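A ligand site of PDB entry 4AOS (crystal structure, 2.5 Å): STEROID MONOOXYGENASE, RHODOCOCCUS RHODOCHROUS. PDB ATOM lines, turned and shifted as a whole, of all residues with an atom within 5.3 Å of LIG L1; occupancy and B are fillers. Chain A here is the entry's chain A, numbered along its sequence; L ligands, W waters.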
ATOM      1  N   ASP A  71       7.465  -8.425 -14.535  1.00  0.00           N
ATOM      2  CA  ASP A  71       7.193  -8.398 -13.088  1.00  0.00           C
ATOM      3  C   ASP A  71       5.767  -7.949 -12.789  1.00  0.00           C
ATOM      4  O   ASP A  71       5.234  -8.230 -11.719  1.00  0.00           O
ATOM      5  CB  ASP A  71       8.111  -7.348 -12.442  1.00  0.00           C
ATOM      6  CG  ASP A  71       9.322  -7.928 -11.792  1.00  0.00           C
ATOM      7  OD1 ASP A  71       9.192  -8.946 -11.064  1.00  0.00           O
ATOM      8  OD2 ASP A  71      10.408  -7.341 -11.973  1.00  0.00           O
ATOM      9  N   LEU A 158      18.107  -0.153 -17.418  1.00  0.00           N
ATOM     10  CA  LEU A 158      18.893  -1.353 -17.159  1.00  0.00           C
ATOM     11  C   LEU A 158      19.869  -1.641 -18.288  1.00  0.00           C
ATOM     12  O   LEU A 158      19.470  -1.938 -19.420  1.00  0.00           O
ATOM     13  CB  LEU A 158      17.962  -2.560 -16.958  1.00  0.00           C
ATOM     14  CG  LEU A 158      17.415  -2.972 -15.598  1.00  0.00           C
ATOM     15  CD1 LEU A 158      16.607  -1.896 -14.903  1.00  0.00           C
ATOM     16  CD2 LEU A 158      16.542  -4.203 -15.766  1.00  0.00           C
ATOM     17  N   PRO A 164      32.176 -10.555 -14.919  1.00  0.00           N
ATOM     18  CA  PRO A 164      33.224 -10.517 -13.892  1.00  0.00           C
ATOM     19  C   PRO A 164      34.486 -11.240 -14.371  1.00  0.00           C
ATOM     20  O   PRO A 164      34.399 -12.230 -15.096  1.00  0.00           O
ATOM     21  CB  PRO A 164      32.599 -11.277 -12.710  1.00  0.00           C
ATOM     22  CG  PRO A 164      31.127 -11.315 -12.992  1.00  0.00           C
ATOM     23  CD  PRO A 164      31.020 -11.357 -14.491  1.00  0.00           C
ATOM     24  N   PHE A 166      37.061 -13.695 -14.381  1.00  0.00           N
ATOM     25  CA  PHE A 166      37.419 -14.997 -13.847  1.00  0.00           C
ATOM     26  C   PHE A 166      38.733 -15.418 -14.476  1.00  0.00           C
ATOM     27  O   PHE A 166      38.903 -15.339 -15.695  1.00  0.00           O
ATOM     28  CB  PHE A 166      36.341 -16.033 -14.134  1.00  0.00           C
ATOM     29  CG  PHE A 166      35.043 -15.784 -13.425  1.00  0.00           C
ATOM     30  CD1 PHE A 166      34.951 -15.954 -12.044  1.00  0.00           C
ATOM     31  CD2 PHE A 166      33.909 -15.372 -14.123  1.00  0.00           C
ATOM     32  CE1 PHE A 166      33.753 -15.720 -11.382  1.00  0.00           C
ATOM     33  CE2 PHE A 166      32.722 -15.132 -13.469  1.00  0.00           C
ATOM     34  CZ  PHE A 166      32.634 -15.309 -12.100  1.00  0.00           C
ATOM     35  N   ILE A 197      26.478 -19.102 -12.681  1.00  0.00           N
ATOM     36  CA  ILE A 197      27.028 -18.117 -11.759  1.00  0.00           C
ATOM     37  C   ILE A 197      26.148 -16.872 -11.812  1.00  0.00           C
ATOM     38  O   ILE A 197      26.007 -16.240 -12.863  1.00  0.00           O
ATOM     39  CB  ILE A 197      28.508 -17.784 -12.093  1.00  0.00           C
ATOM     40  CG1 ILE A 197      29.334 -19.069 -12.216  1.00  0.00           C
ATOM     41  CG2 ILE A 197      29.112 -16.874 -11.039  1.00  0.00           C
ATOM     42  CD1 ILE A 197      30.652 -18.906 -12.954  1.00  0.00           C
ATOM     43  N   GLY A 198      25.532 -16.557 -10.681  1.00  0.00           N
ATOM     44  CA  GLY A 198      24.617 -15.420 -10.575  1.00  0.00           C
ATOM     45  C   GLY A 198      23.210 -15.837 -10.201  1.00  0.00           C
ATOM     46  O   GLY A 198      22.597 -16.659 -10.880  1.00  0.00           O
ATOM     47  N   THR A 199      22.704 -15.268  -9.113  1.00  0.00           N
ATOM     48  CA  THR A 199      21.353 -15.587  -8.654  1.00  0.00           C
ATOM     49  C   THR A 199      20.460 -14.335  -8.513  1.00  0.00           C
ATOM     50  O   THR A 199      19.606 -14.272  -7.634  1.00  0.00           O
ATOM     51  CB  THR A 199      21.370 -16.418  -7.336  1.00  0.00           C
ATOM     52  OG1 THR A 199      22.121 -15.713  -6.321  1.00  0.00           O
ATOM     53  CG2 THR A 199      22.013 -17.778  -7.558  1.00  0.00           C
ATOM     54  N   GLY A 200      20.677 -13.345  -9.373  1.00  0.00           N
ATOM     55  CA  GLY A 200      19.730 -12.246  -9.521  1.00  0.00           C
ATOM     56  C   GLY A 200      18.612 -12.706 -10.453  1.00  0.00           C
ATOM     57  O   GLY A 200      18.420 -13.909 -10.646  1.00  0.00           O
ATOM     58  N   SER A 201      17.889 -11.764 -11.056  1.00  0.00           N
ATOM     59  CA  SER A 201      16.717 -12.154 -11.825  1.00  0.00           C
ATOM     60  C   SER A 201      17.016 -13.049 -13.033  1.00  0.00           C
ATOM     61  O   SER A 201      16.225 -13.919 -13.358  1.00  0.00           O
ATOM     62  CB  SER A 201      15.869 -10.937 -12.218  1.00  0.00           C
ATOM     63  OG  SER A 201      16.544 -10.170 -13.181  1.00  0.00           O
ATOM     64  N   SER A 202      18.149 -12.837 -13.694  1.00  0.00           N
ATOM     65  CA  SER A 202      18.543 -13.665 -14.851  1.00  0.00           C
ATOM     66  C   SER A 202      18.807 -15.125 -14.478  1.00  0.00           C
ATOM     67  O   SER A 202      18.485 -16.036 -15.246  1.00  0.00           O
ATOM     68  CB  SER A 202      19.786 -13.083 -15.522  1.00  0.00           C
ATOM     69  OG  SER A 202      19.445 -11.851 -16.120  1.00  0.00           O
ATOM     70  N   PHE A 220      25.955 -21.604  -8.393  1.00  0.00           N
ATOM     71  CA  PHE A 220      26.998 -21.023  -7.586  1.00  0.00           C
ATOM     72  C   PHE A 220      26.510 -19.698  -7.011  1.00  0.00           C
ATOM     73  O   PHE A 220      26.538 -18.667  -7.683  1.00  0.00           O
ATOM     74  CB  PHE A 220      28.277 -20.842  -8.405  1.00  0.00           C
ATOM     75  CG  PHE A 220      28.887 -22.132  -8.872  1.00  0.00           C
ATOM     76  CD1 PHE A 220      28.497 -22.712 -10.079  1.00  0.00           C
ATOM     77  CD2 PHE A 220      29.847 -22.787  -8.102  1.00  0.00           C
ATOM     78  CE1 PHE A 220      29.061 -23.906 -10.510  1.00  0.00           C
ATOM     79  CE2 PHE A 220      30.410 -23.983  -8.523  1.00  0.00           C
ATOM     80  CZ  PHE A 220      30.013 -24.543  -9.737  1.00  0.00           C
ATOM     81  N   ARG A 222      26.383 -16.601  -4.226  1.00  0.00           N
ATOM     82  CA  ARG A 222      27.129 -15.774  -3.290  1.00  0.00           C
ATOM     83  C   ARG A 222      26.183 -15.086  -2.294  1.00  0.00           C
ATOM     84  O   ARG A 222      26.401 -15.145  -1.093  1.00  0.00           O
ATOM     85  CB  ARG A 222      28.000 -14.749  -4.023  1.00  0.00           C
ATOM     86  CG  ARG A 222      29.117 -14.156  -3.157  1.00  0.00           C
ATOM     87  CD  ARG A 222      30.177 -13.400  -3.960  1.00  0.00           C
ATOM     88  NE  ARG A 222      29.601 -12.317  -4.758  1.00  0.00           N
ATOM     89  CZ  ARG A 222      30.318 -11.467  -5.507  1.00  0.00           C
ATOM     90  NH1 ARG A 222      31.639 -11.571  -5.562  1.00  0.00           N
ATOM     91  NH2 ARG A 222      29.695 -10.521  -6.203  1.00  0.00           N
ATOM     92  N   SER A 223      25.129 -14.460  -2.810  1.00  0.00           N
ATOM     93  CA  SER A 223      24.114 -13.807  -1.979  1.00  0.00           C
ATOM     94  C   SER A 223      22.733 -14.264  -2.429  1.00  0.00           C
ATOM     95  O   SER A 223      22.369 -14.077  -3.595  1.00  0.00           O
ATOM     96  CB  SER A 223      24.199 -12.280  -2.098  1.00  0.00           C
ATOM     97  OG  SER A 223      25.486 -11.786  -1.781  1.00  0.00           O
ATOM     98  N   ASN A 225      18.788 -13.976  -2.872  1.00  0.00           N
ATOM     99  CA  ASN A 225      17.843 -12.889  -3.074  1.00  0.00           C
ATOM    100  C   ASN A 225      16.400 -13.321  -2.777  1.00  0.00           C
ATOM    101  O   ASN A 225      16.094 -14.524  -2.804  1.00  0.00           O
ATOM    102  CB  ASN A 225      17.920 -12.375  -4.499  1.00  0.00           C
ATOM    103  CG  ASN A 225      19.217 -11.642  -4.798  1.00  0.00           C
ATOM    104  OD1 ASN A 225      19.805 -11.814  -5.862  1.00  0.00           O
ATOM    105  ND2 ASN A 225      19.652 -10.811  -3.854  1.00  0.00           N
ATOM    106  N   LYS A 341      16.122  -4.272  -2.080  1.00  0.00           N
ATOM    107  CA  LYS A 341      16.471  -4.678  -3.434  1.00  0.00           C
ATOM    108  C   LYS A 341      15.167  -5.207  -4.045  1.00  0.00           C
ATOM    109  O   LYS A 341      14.360  -5.825  -3.339  1.00  0.00           O
ATOM    110  CB  LYS A 341      17.571  -5.737  -3.388  1.00  0.00           C
ATOM    111  CG  LYS A 341      17.907  -6.385  -4.719  1.00  0.00           C
ATOM    112  CD  LYS A 341      19.406  -6.633  -4.901  1.00  0.00           C
ATOM    113  CE  LYS A 341      19.979  -7.687  -3.954  1.00  0.00           C
ATOM    114  NZ  LYS A 341      20.366  -7.116  -2.635  1.00  0.00           N
ATOM    115  N   ARG A 342      14.945  -4.947  -5.339  1.00  0.00           N
ATOM    116  CA  ARG A 342      13.693  -5.331  -5.959  1.00  0.00           C
ATOM    117  C   ARG A 342      13.486  -6.838  -5.886  1.00  0.00           C
ATOM    118  O   ARG A 342      14.377  -7.617  -6.220  1.00  0.00           O
ATOM    119  CB  ARG A 342      13.612  -4.848  -7.413  1.00  0.00           C
ATOM    120  CG  ARG A 342      12.225  -4.939  -8.026  1.00  0.00           C
ATOM    121  CD  ARG A 342      12.306  -4.851  -9.536  1.00  0.00           C
ATOM    122  NE  ARG A 342      11.008  -4.815 -10.208  1.00  0.00           N
ATOM    123  CZ  ARG A 342      10.380  -3.694 -10.574  1.00  0.00           C
ATOM    124  NH1 ARG A 342      10.927  -2.500 -10.316  1.00  0.00           N
ATOM    125  NH2 ARG A 342       9.203  -3.755 -11.206  1.00  0.00           N
ATOM    126  N   LEU A 363      29.076 -19.945  -2.227  1.00  0.00           N
ATOM    127  CA  LEU A 363      30.344 -19.304  -2.587  1.00  0.00           C
ATOM    128  C   LEU A 363      30.995 -18.546  -1.426  1.00  0.00           C
ATOM    129  O   LEU A 363      32.155 -18.139  -1.524  1.00  0.00           O
ATOM    130  CB  LEU A 363      30.170 -18.391  -3.819  1.00  0.00           C
ATOM    131  CG  LEU A 363      29.888 -19.042  -5.176  1.00  0.00           C
ATOM    132  CD1 LEU A 363      29.746 -17.993  -6.276  1.00  0.00           C
ATOM    133  CD2 LEU A 363      30.934 -20.097  -5.563  1.00  0.00           C
ATOM    134  N   ARG A 364      30.262 -18.353  -0.339  1.00  0.00           N
ATOM    135  CA  ARG A 364      30.836 -17.770   0.873  1.00  0.00           C
ATOM    136  C   ARG A 364      31.679 -18.834   1.594  1.00  0.00           C
ATOM    137  O   ARG A 364      32.672 -18.509   2.213  1.00  0.00           O
ATOM    138  CB  ARG A 364      29.748 -17.188   1.797  1.00  0.00           C
ATOM    139  CG  ARG A 364      28.678 -16.409   1.054  1.00  0.00           C
ATOM    140  CD  ARG A 364      28.659 -14.896   1.283  1.00  0.00           C
ATOM    141  NE  ARG A 364      29.829 -14.175   0.778  1.00  0.00           N
ATOM    142  CZ  ARG A 364      29.790 -12.969   0.207  1.00  0.00           C
ATOM    143  NH1 ARG A 364      28.631 -12.343   0.010  1.00  0.00           N
ATOM    144  NH2 ARG A 364      30.908 -12.396  -0.208  1.00  0.00           N
ATOM    145  N   ILE A 368      34.726 -19.064  -5.963  1.00  0.00           N
ATOM    146  CA  ILE A 368      35.380 -19.395  -7.227  1.00  0.00           C
ATOM    147  C   ILE A 368      36.754 -18.719  -7.246  1.00  0.00           C
ATOM    148  O   ILE A 368      36.851 -17.507  -7.028  1.00  0.00           O
ATOM    149  CB  ILE A 368      34.536 -18.958  -8.441  1.00  0.00           C
ATOM    150  CG1 ILE A 368      33.248 -19.799  -8.531  1.00  0.00           C
ATOM    151  CG2 ILE A 368      35.340 -19.085  -9.735  1.00  0.00           C
ATOM    152  CD1 ILE A 368      32.138 -19.100  -9.303  1.00  0.00           C
ATOM    153  N   ALA A 391      25.099 -15.641 -15.418  1.00  0.00           N
ATOM    154  CA  ALA A 391      23.838 -14.951 -15.202  1.00  0.00           C
ATOM    155  C   ALA A 391      24.151 -13.585 -14.610  1.00  0.00           C
ATOM    156  O   ALA A 391      24.021 -13.334 -13.404  1.00  0.00           O
ATOM    157  CB  ALA A 391      22.913 -15.752 -14.306  1.00  0.00           C
ATOM    158  N   THR A 392      24.601 -12.696 -15.503  1.00  0.00           N
ATOM    159  CA  THR A 392      25.081 -11.384 -15.135  1.00  0.00           C
ATOM    160  C   THR A 392      23.932 -10.513 -14.649  1.00  0.00           C
ATOM    161  O   THR A 392      22.753 -10.734 -14.985  1.00  0.00           O
ATOM    162  CB  THR A 392      25.771 -10.674 -16.312  1.00  0.00           C
ATOM    163  OG1 THR A 392      24.910 -10.718 -17.469  1.00  0.00           O
ATOM    164  CG2 THR A 392      27.098 -11.351 -16.633  1.00  0.00           C
ATOM    165  N   GLY A 393      24.310  -9.518 -13.839  1.00  0.00           N
ATOM    166  CA  GLY A 393      23.386  -8.520 -13.383  1.00  0.00           C
ATOM    167  C   GLY A 393      23.418  -7.288 -14.260  1.00  0.00           C
ATOM    168  O   GLY A 393      23.992  -7.287 -15.341  1.00  0.00           O
ATOM    169  N   PHE A 394      22.782  -6.237 -13.761  1.00  0.00           N
ATOM    170  CA  PHE A 394      22.599  -5.010 -14.512  1.00  0.00           C
ATOM    171  C   PHE A 394      23.333  -3.849 -13.827  1.00  0.00           C
ATOM    172  O   PHE A 394      23.318  -3.727 -12.597  1.00  0.00           O
ATOM    173  CB  PHE A 394      21.106  -4.724 -14.679  1.00  0.00           C
ATOM    174  CG  PHE A 394      20.369  -5.796 -15.438  1.00  0.00           C
ATOM    175  CD1 PHE A 394      20.334  -5.791 -16.830  1.00  0.00           C
ATOM    176  CD2 PHE A 394      19.721  -6.834 -14.773  1.00  0.00           C
ATOM    177  CE1 PHE A 394      19.666  -6.786 -17.538  1.00  0.00           C
ATOM    178  CE2 PHE A 394      19.056  -7.840 -15.473  1.00  0.00           C
ATOM    179  CZ  PHE A 394      19.031  -7.811 -16.849  1.00  0.00           C
ATOM    180  N   VAL A 447      12.204   3.023 -12.351  1.00  0.00           N
ATOM    181  CA  VAL A 447      11.924   1.595 -12.156  1.00  0.00           C
ATOM    182  C   VAL A 447      10.983   1.287 -10.999  1.00  0.00           C
ATOM    183  O   VAL A 447      10.516   0.174 -10.867  1.00  0.00           O
ATOM    184  CB  VAL A 447      13.224   0.769 -11.978  1.00  0.00           C
ATOM    185  CG1 VAL A 447      13.963   0.652 -13.305  1.00  0.00           C
ATOM    186  CG2 VAL A 447      14.124   1.349 -10.885  1.00  0.00           C
ATOM    187  N   TRP A 506      20.971  -0.490  -4.911  1.00  0.00           N
ATOM    188  CA  TRP A 506      21.126  -0.217  -6.338  1.00  0.00           C
ATOM    189  C   TRP A 506      20.538   1.098  -6.764  1.00  0.00           C
ATOM    190  O   TRP A 506      20.979   1.679  -7.760  1.00  0.00           O
ATOM    191  CB  TRP A 506      20.540  -1.369  -7.153  1.00  0.00           C
ATOM    192  CG  TRP A 506      20.720  -1.207  -8.651  1.00  0.00           C
ATOM    193  CD1 TRP A 506      21.842  -1.515  -9.405  1.00  0.00           C
ATOM    194  CD2 TRP A 506      19.731  -0.698  -9.615  1.00  0.00           C
ATOM    195  NE1 TRP A 506      21.628  -1.234 -10.735  1.00  0.00           N
ATOM    196  CE2 TRP A 506      20.384  -0.744 -10.935  1.00  0.00           C
ATOM    197  CE3 TRP A 506      18.418  -0.231  -9.528  1.00  0.00           C
ATOM    198  CZ2 TRP A 506      19.737  -0.329 -12.087  1.00  0.00           C
ATOM    199  CZ3 TRP A 506      17.777   0.180 -10.711  1.00  0.00           C
ATOM    200  CH2 TRP A 506      18.421   0.130 -11.961  1.00  0.00           C
ATOM    201  N   TYR A 507      19.554   1.600  -6.012  1.00  0.00           N
ATOM    202  CA  TYR A 507      18.934   2.891  -6.312  1.00  0.00           C
ATOM    203  C   TYR A 507      19.834   4.069  -5.888  1.00  0.00           C
ATOM    204  O   TYR A 507      19.422   5.231  -5.994  1.00  0.00           O
ATOM    205  CB  TYR A 507      17.546   3.029  -5.642  1.00  0.00           C
ATOM    206  CG  TYR A 507      16.553   1.919  -5.928  1.00  0.00           C
ATOM    207  CD1 TYR A 507      15.935   1.798  -7.174  1.00  0.00           C
ATOM    208  CD2 TYR A 507      16.211   0.997  -4.941  1.00  0.00           C
ATOM    209  CE1 TYR A 507      15.022   0.775  -7.435  1.00  0.00           C
ATOM    210  CE2 TYR A 507      15.302  -0.017  -5.180  1.00  0.00           C
ATOM    211  CZ  TYR A 507      14.713  -0.125  -6.431  1.00  0.00           C
ATOM    212  OH  TYR A 507      13.804  -1.139  -6.670  1.00  0.00           O
HETATM  213  P1  LIG L   1      21.893  -8.882  -8.782  1.00  0.00           P
HETATM  214  O1  LIG L   1      20.582  -9.177  -8.090  1.00  0.00           O
HETATM  215  O2  LIG L   1      23.110  -8.553  -7.930  1.00  0.00           O
HETATM  216  O3  LIG L   1      22.279 -10.076  -9.819  1.00  0.00           O
HETATM  217  C1  LIG L   1      23.629 -10.390 -10.200  1.00  0.00           C
HETATM  218  C2  LIG L   1      24.079 -11.729  -9.594  1.00  0.00           C
HETATM  219  O4  LIG L   1      25.390 -12.140 -10.028  1.00  0.00           O
HETATM  220  C3  LIG L   1      24.156 -11.648  -8.079  1.00  0.00           C
HETATM  221  O5  LIG L   1      23.679 -12.886  -7.554  1.00  0.00           O
HETATM  222  C4  LIG L   1      25.633 -11.481  -7.823  1.00  0.00           C
HETATM  223  O6  LIG L   1      26.027 -11.825  -6.502  1.00  0.00           O
HETATM  224  C5  LIG L   1      26.214 -12.398  -8.882  1.00  0.00           C
HETATM  225  N1  LIG L   1      27.639 -12.049  -9.125  1.00  0.00           N
HETATM  226  C6  LIG L   1      28.114 -10.910  -9.661  1.00  0.00           C
HETATM  227  N2  LIG L   1      29.464 -10.942  -9.740  1.00  0.00           N
HETATM  228  C7  LIG L   1      29.877 -12.126  -9.239  1.00  0.00           C
HETATM  229  C8  LIG L   1      31.179 -12.814  -9.023  1.00  0.00           C
HETATM  230  N3  LIG L   1      32.347 -12.231  -9.361  1.00  0.00           N
HETATM  231  N4  LIG L   1      31.162 -14.064  -8.465  1.00  0.00           N
HETATM  232  C9  LIG L   1      30.001 -14.667  -8.120  1.00  0.00           C
HETATM  233  N5  LIG L   1      28.796 -14.098  -8.291  1.00  0.00           N
HETATM  234  C10 LIG L   1      28.672 -12.858  -8.831  1.00  0.00           C
HETATM  235  O7  LIG L   1      21.663  -7.635  -9.778  1.00  0.00           O
HETATM  236  P2  LIG L   1      20.516  -7.633 -10.906  1.00  0.00           P
HETATM  237  O8  LIG L   1      19.621  -8.845 -10.785  1.00  0.00           O
HETATM  238  O9  LIG L   1      21.208  -7.315 -12.181  1.00  0.00           O
HETATM  239  O10 LIG L   1      19.634  -6.340 -10.520  1.00  0.00           O
HETATM  240  C11 LIG L   1      20.267  -5.144 -10.051  1.00  0.00           C
HETATM  241  C12 LIG L   1      19.208  -4.080  -9.816  1.00  0.00           C
HETATM  242  O11 LIG L   1      18.505  -3.823 -11.034  1.00  0.00           O
HETATM  243  C13 LIG L   1      18.179  -4.494  -8.790  1.00  0.00           C
HETATM  244  O12 LIG L   1      18.507  -3.955  -7.503  1.00  0.00           O
HETATM  245  C14 LIG L   1      16.869  -3.956  -9.323  1.00  0.00           C
HETATM  246  O13 LIG L   1      16.527  -2.703  -8.720  1.00  0.00           O
HETATM  247  C15 LIG L   1      17.098  -3.707 -10.810  1.00  0.00           C
HETATM  248  N6  LIG L   1      16.282  -4.615 -11.644  1.00  0.00           N
HETATM  249  C16 LIG L   1      15.045  -4.220 -11.986  1.00  0.00           C
HETATM  250  C17 LIG L   1      14.211  -5.020 -12.780  1.00  0.00           C
HETATM  251  C18 LIG L   1      12.832  -4.541 -13.135  1.00  0.00           C
HETATM  252  O14 LIG L   1      12.595  -3.343 -13.191  1.00  0.00           O
HETATM  253  N7  LIG L   1      11.889  -5.450 -13.366  1.00  0.00           N
HETATM  254  C19 LIG L   1      14.684  -6.250 -13.235  1.00  0.00           C
HETATM  255  C20 LIG L   1      15.974  -6.646 -12.880  1.00  0.00           C
HETATM  256  C21 LIG L   1      16.757  -5.803 -12.081  1.00  0.00           C
HETATM  257  P3  LIG L   1      26.236 -10.668  -5.388  1.00  0.00           P
HETATM  258  O15 LIG L   1      27.101  -9.639  -6.089  1.00  0.00           O
HETATM  259  O16 LIG L   1      24.829 -10.192  -5.071  1.00  0.00           O
HETATM  260  O17 LIG L   1      26.932 -11.379  -4.250  1.00  0.00           O
HETATM  261  P1  LG2 L   2      14.999  -0.262 -22.959  1.00  0.00           P
HETATM  262  O1  LG2 L   2      14.045  -1.408 -23.054  1.00  0.00           O
HETATM  263  O2  LG2 L   2      16.288  -0.513 -22.217  1.00  0.00           O
HETATM  264  O3  LG2 L   2      15.283   0.294 -24.422  1.00  0.00           O
HETATM  265  C1  LG2 L   2      16.326   1.249 -24.603  1.00  0.00           C
HETATM  266  C2  LG2 L   2      17.062   0.971 -25.902  1.00  0.00           C
HETATM  267  O4  LG2 L   2      18.015   2.006 -26.136  1.00  0.00           O
HETATM  268  C3  LG2 L   2      17.853  -0.326 -25.907  1.00  0.00           C
HETATM  269  O5  LG2 L   2      17.489  -0.993 -27.119  1.00  0.00           O
HETATM  270  C4  LG2 L   2      19.301   0.058 -26.039  1.00  0.00           C
HETATM  271  O6  LG2 L   2      19.942  -0.859 -26.930  1.00  0.00           O
HETATM  272  C5  LG2 L   2      19.189   1.424 -26.705  1.00  0.00           C
HETATM  273  N1  LG2 L   2      20.344   2.313 -26.452  1.00  0.00           N
HETATM  274  C6  LG2 L   2      20.909   2.607 -25.257  1.00  0.00           C
HETATM  275  N2  LG2 L   2      21.933   3.474 -25.427  1.00  0.00           N
HETATM  276  C7  LG2 L   2      22.031   3.735 -26.738  1.00  0.00           C
HETATM  277  C8  LG2 L   2      22.897   4.559 -27.603  1.00  0.00           C
HETATM  278  N3  LG2 L   2      23.892   5.308 -27.073  1.00  0.00           N
HETATM  279  N4  LG2 L   2      22.670   4.559 -28.939  1.00  0.00           N
HETATM  280  C9  LG2 L   2      21.672   3.821 -29.478  1.00  0.00           C
HETATM  281  N5  LG2 L   2      20.849   3.050 -28.752  1.00  0.00           N
HETATM  282  C10 LG2 L   2      20.972   2.981 -27.407  1.00  0.00           C
HETATM  283  N6  LG2 L   2       9.694  -2.890 -15.976  1.00  0.00           N
HETATM  284  C11 LG2 L   2       8.395  -2.752 -15.596  1.00  0.00           C
HETATM  285  O7  LG2 L   2       7.897  -1.599 -15.475  1.00  0.00           O
HETATM  286  N7  LG2 L   2       7.614  -3.813 -15.344  1.00  0.00           N
HETATM  287  C12 LG2 L   2       8.055  -5.072 -15.449  1.00  0.00           C
HETATM  288  O8  LG2 L   2       7.305  -6.037 -15.227  1.00  0.00           O
HETATM  289  C13 LG2 L   2       9.455  -5.317 -15.843  1.00  0.00           C
HETATM  290  N8  LG2 L   2       9.951  -6.571 -15.963  1.00  0.00           N
HETATM  291  C14 LG2 L   2      11.242  -6.747 -16.331  1.00  0.00           C
HETATM  292  C15 LG2 L   2      11.734  -8.048 -16.441  1.00  0.00           C
HETATM  293  C16 LG2 L   2      13.054  -8.266 -16.815  1.00  0.00           C
HETATM  294  C17 LG2 L   2      13.561  -9.682 -16.926  1.00  0.00           C
HETATM  295  C18 LG2 L   2      13.952  -7.102 -17.109  1.00  0.00           C
HETATM  296  C19 LG2 L   2      15.384  -7.288 -17.509  1.00  0.00           C
HETATM  297  C20 LG2 L   2      13.459  -5.802 -16.989  1.00  0.00           C
HETATM  298  C21 LG2 L   2      12.135  -5.578 -16.604  1.00  0.00           C
HETATM  299  N9  LG2 L   2      11.608  -4.268 -16.506  1.00  0.00           N
HETATM  300  C22 LG2 L   2      10.269  -4.116 -16.116  1.00  0.00           C
HETATM  301  C23 LG2 L   2      12.431  -3.062 -16.715  1.00  0.00           C
HETATM  302  C24 LG2 L   2      12.650  -2.747 -18.169  1.00  0.00           C
HETATM  303  O9  LG2 L   2      14.048  -2.487 -18.279  1.00  0.00           O
HETATM  304  C25 LG2 L   2      11.843  -1.522 -18.569  1.00  0.00           C
HETATM  305  O10 LG2 L   2      10.448  -1.795 -18.370  1.00  0.00           O
HETATM  306  C26 LG2 L   2      12.018  -1.201 -20.036  1.00  0.00           C
HETATM  307  O11 LG2 L   2      13.377  -1.396 -20.443  1.00  0.00           O
HETATM  308  C27 LG2 L   2      11.608   0.218 -20.346  1.00  0.00           C
HETATM  309  O12 LG2 L   2      11.876   0.389 -21.734  1.00  0.00           O
HETATM  310  P2  LG2 L   2      12.809   1.568 -22.288  1.00  0.00           P
HETATM  311  O13 LG2 L   2      12.439   1.820 -23.727  1.00  0.00           O
HETATM  312  O14 LG2 L   2      12.783   2.672 -21.283  1.00  0.00           O
HETATM  313  O15 LG2 L   2      14.331   1.011 -22.213  1.00  0.00           O
HETATM  314  O   HOH W   1      20.239 -10.778 -13.015  1.00  0.00           O
HETATM  315  O   HOH W   2      14.364  -1.950  -9.683  1.00  0.00           O
HETATM  316  O   HOH W   3      19.497  -2.466  -4.515  1.00  0.00           O
HETATM  317  O   HOH W   4      24.506  -6.702  -9.236  1.00  0.00           O
HETATM  318  O   HOH W   5      26.701 -15.895  -7.967  1.00  0.00           O
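The backbone NH (N) of Phe 394 is in hydrogen-bond range of an oxygen (O9) of LIG L1, 2.5 Å away. The guanidinium group of Arg 222 lies within salt-bridge range of an oxygen (O15) of LIG L1 (2.7 Å). OD2 of Asp 71 is in hydrogen-bond range of N7 of LIG L1 (2.8 Å). O17 of LIG L1 sits at hydrogen-bond distance from OG of Ser 223, at 2.9 Å. N of Thr 199 is in hydrogen-bond range of O5 of LIG L1, at 3.0 Å. An oxygen (O5) of LIG L1 lies within hydrogen-bond range of the side-chain hydroxyl (OG1) of Thr 199 (3.5 Å). NH1 of Arg 342 is in hydrogen-bond range of O14 of LIG L1, at 3.4 Å. N of Ser 201 lies within hydrogen-bond range of O8 of LIG L1, 3.4 Å away. The backbone NH (N) of Asp 71 is in hydrogen-bond range of an oxygen (O8) of LG2 L2 (2.5 Å).
A nitrogen (N8) of LG2 L2 lies close to a nitrogen (N7) of LIG L1, 3.4 Å away.
The guanidinium group of Arg 342 lies within salt-bridge range of the side-chain carboxylate of Asp 71, 3.1 Å away. The side-chain hydroxyl (OG1) of Thr 199 sits at hydrogen-bond distance from the backbone carbonyl oxygen (O) of Ser 223 (3.2 Å). The backbone carbonyl oxygen (O) of Thr 199 sits close to the side-chain amide oxygen (OD1) of Asn 225, 3.0 Å away. NH1 of Arg 342 lies within hydrogen-bond range of O of Val 447, at 2.8 Å. The backbone NH (N) of Ala 391 lies within hydrogen-bond range of the backbone carbonyl oxygen (O) of Ile 197, at 2.8 Å.
Leu 158 touches LIG L1 (CD2 to C19, 3.7 Å). Pro 164 touches LIG L1 (CB to N3, 3.5 Å). Ile 197 touches LIG L1. CA of Gly 198 touches O4 of LIG L1 (3.4 Å). Gly 200 touches LIG L1. OD1 of Asn 225 touches O1 of LIG L1, 3.5 Å away. CG of Lys 341 touches O12 of LIG L1 (3.7 Å). Leu 363 touches LIG L1 (CD1 to C9, 3.8 Å). O of Ala 391 touches O4 of LIG L1, 3.8 Å away. Gly 393 touches LIG L1 (CA to O9, 2.8 Å). CE3 of Trp 506 touches O13 of LIG L1, 3.2 Å away. Tyr 507 touches LIG L1. Hydrophobic or aromatic side chains within 4 Å of LIG L1: Leu 158, Pro 164, Ile 197, Leu 363, Phe 394, Trp 506 and Tyr 507. 19 residues have an atom within 4 Å of LIG L1: Asp 71, Leu 158, Pro 164, Ile 197, Gly 198, Thr 199, Gly 200, Ser 201, Arg 222, Ser 223, Asn 225, Lys 341, Arg 342, Leu 363, Ala 391, Gly 393, Phe 394, Trp 506 and Tyr 507. The nearest printed residue that does not touch LIG L1 is Phe 166 (4.1 Å).
Water W2 lies within hydrogen-bond range of an oxygen (O13) of LIG L1 and the side-chain hydroxyl (OH) of Tyr 507. Water W5 lies within hydrogen-bond range of N5 of LIG L1 (2.8 Å), O of Phe 220 (2.8 Å) and N of Gly 198 (3.0 Å). Water W1 lies within hydrogen-bond range of the backbone NH of Ser 202 (3.0 Å), an oxygen (O8) of LIG L1 (3.0 Å), the backbone carbonyl oxygen of Thr 392 (3.2 Å) and the backbone NH of Ser 201 (3.2 Å). Water W3 bridges N of Trp 506 (2.5 Å) and O12 of LIG L1 (3.5 Å).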
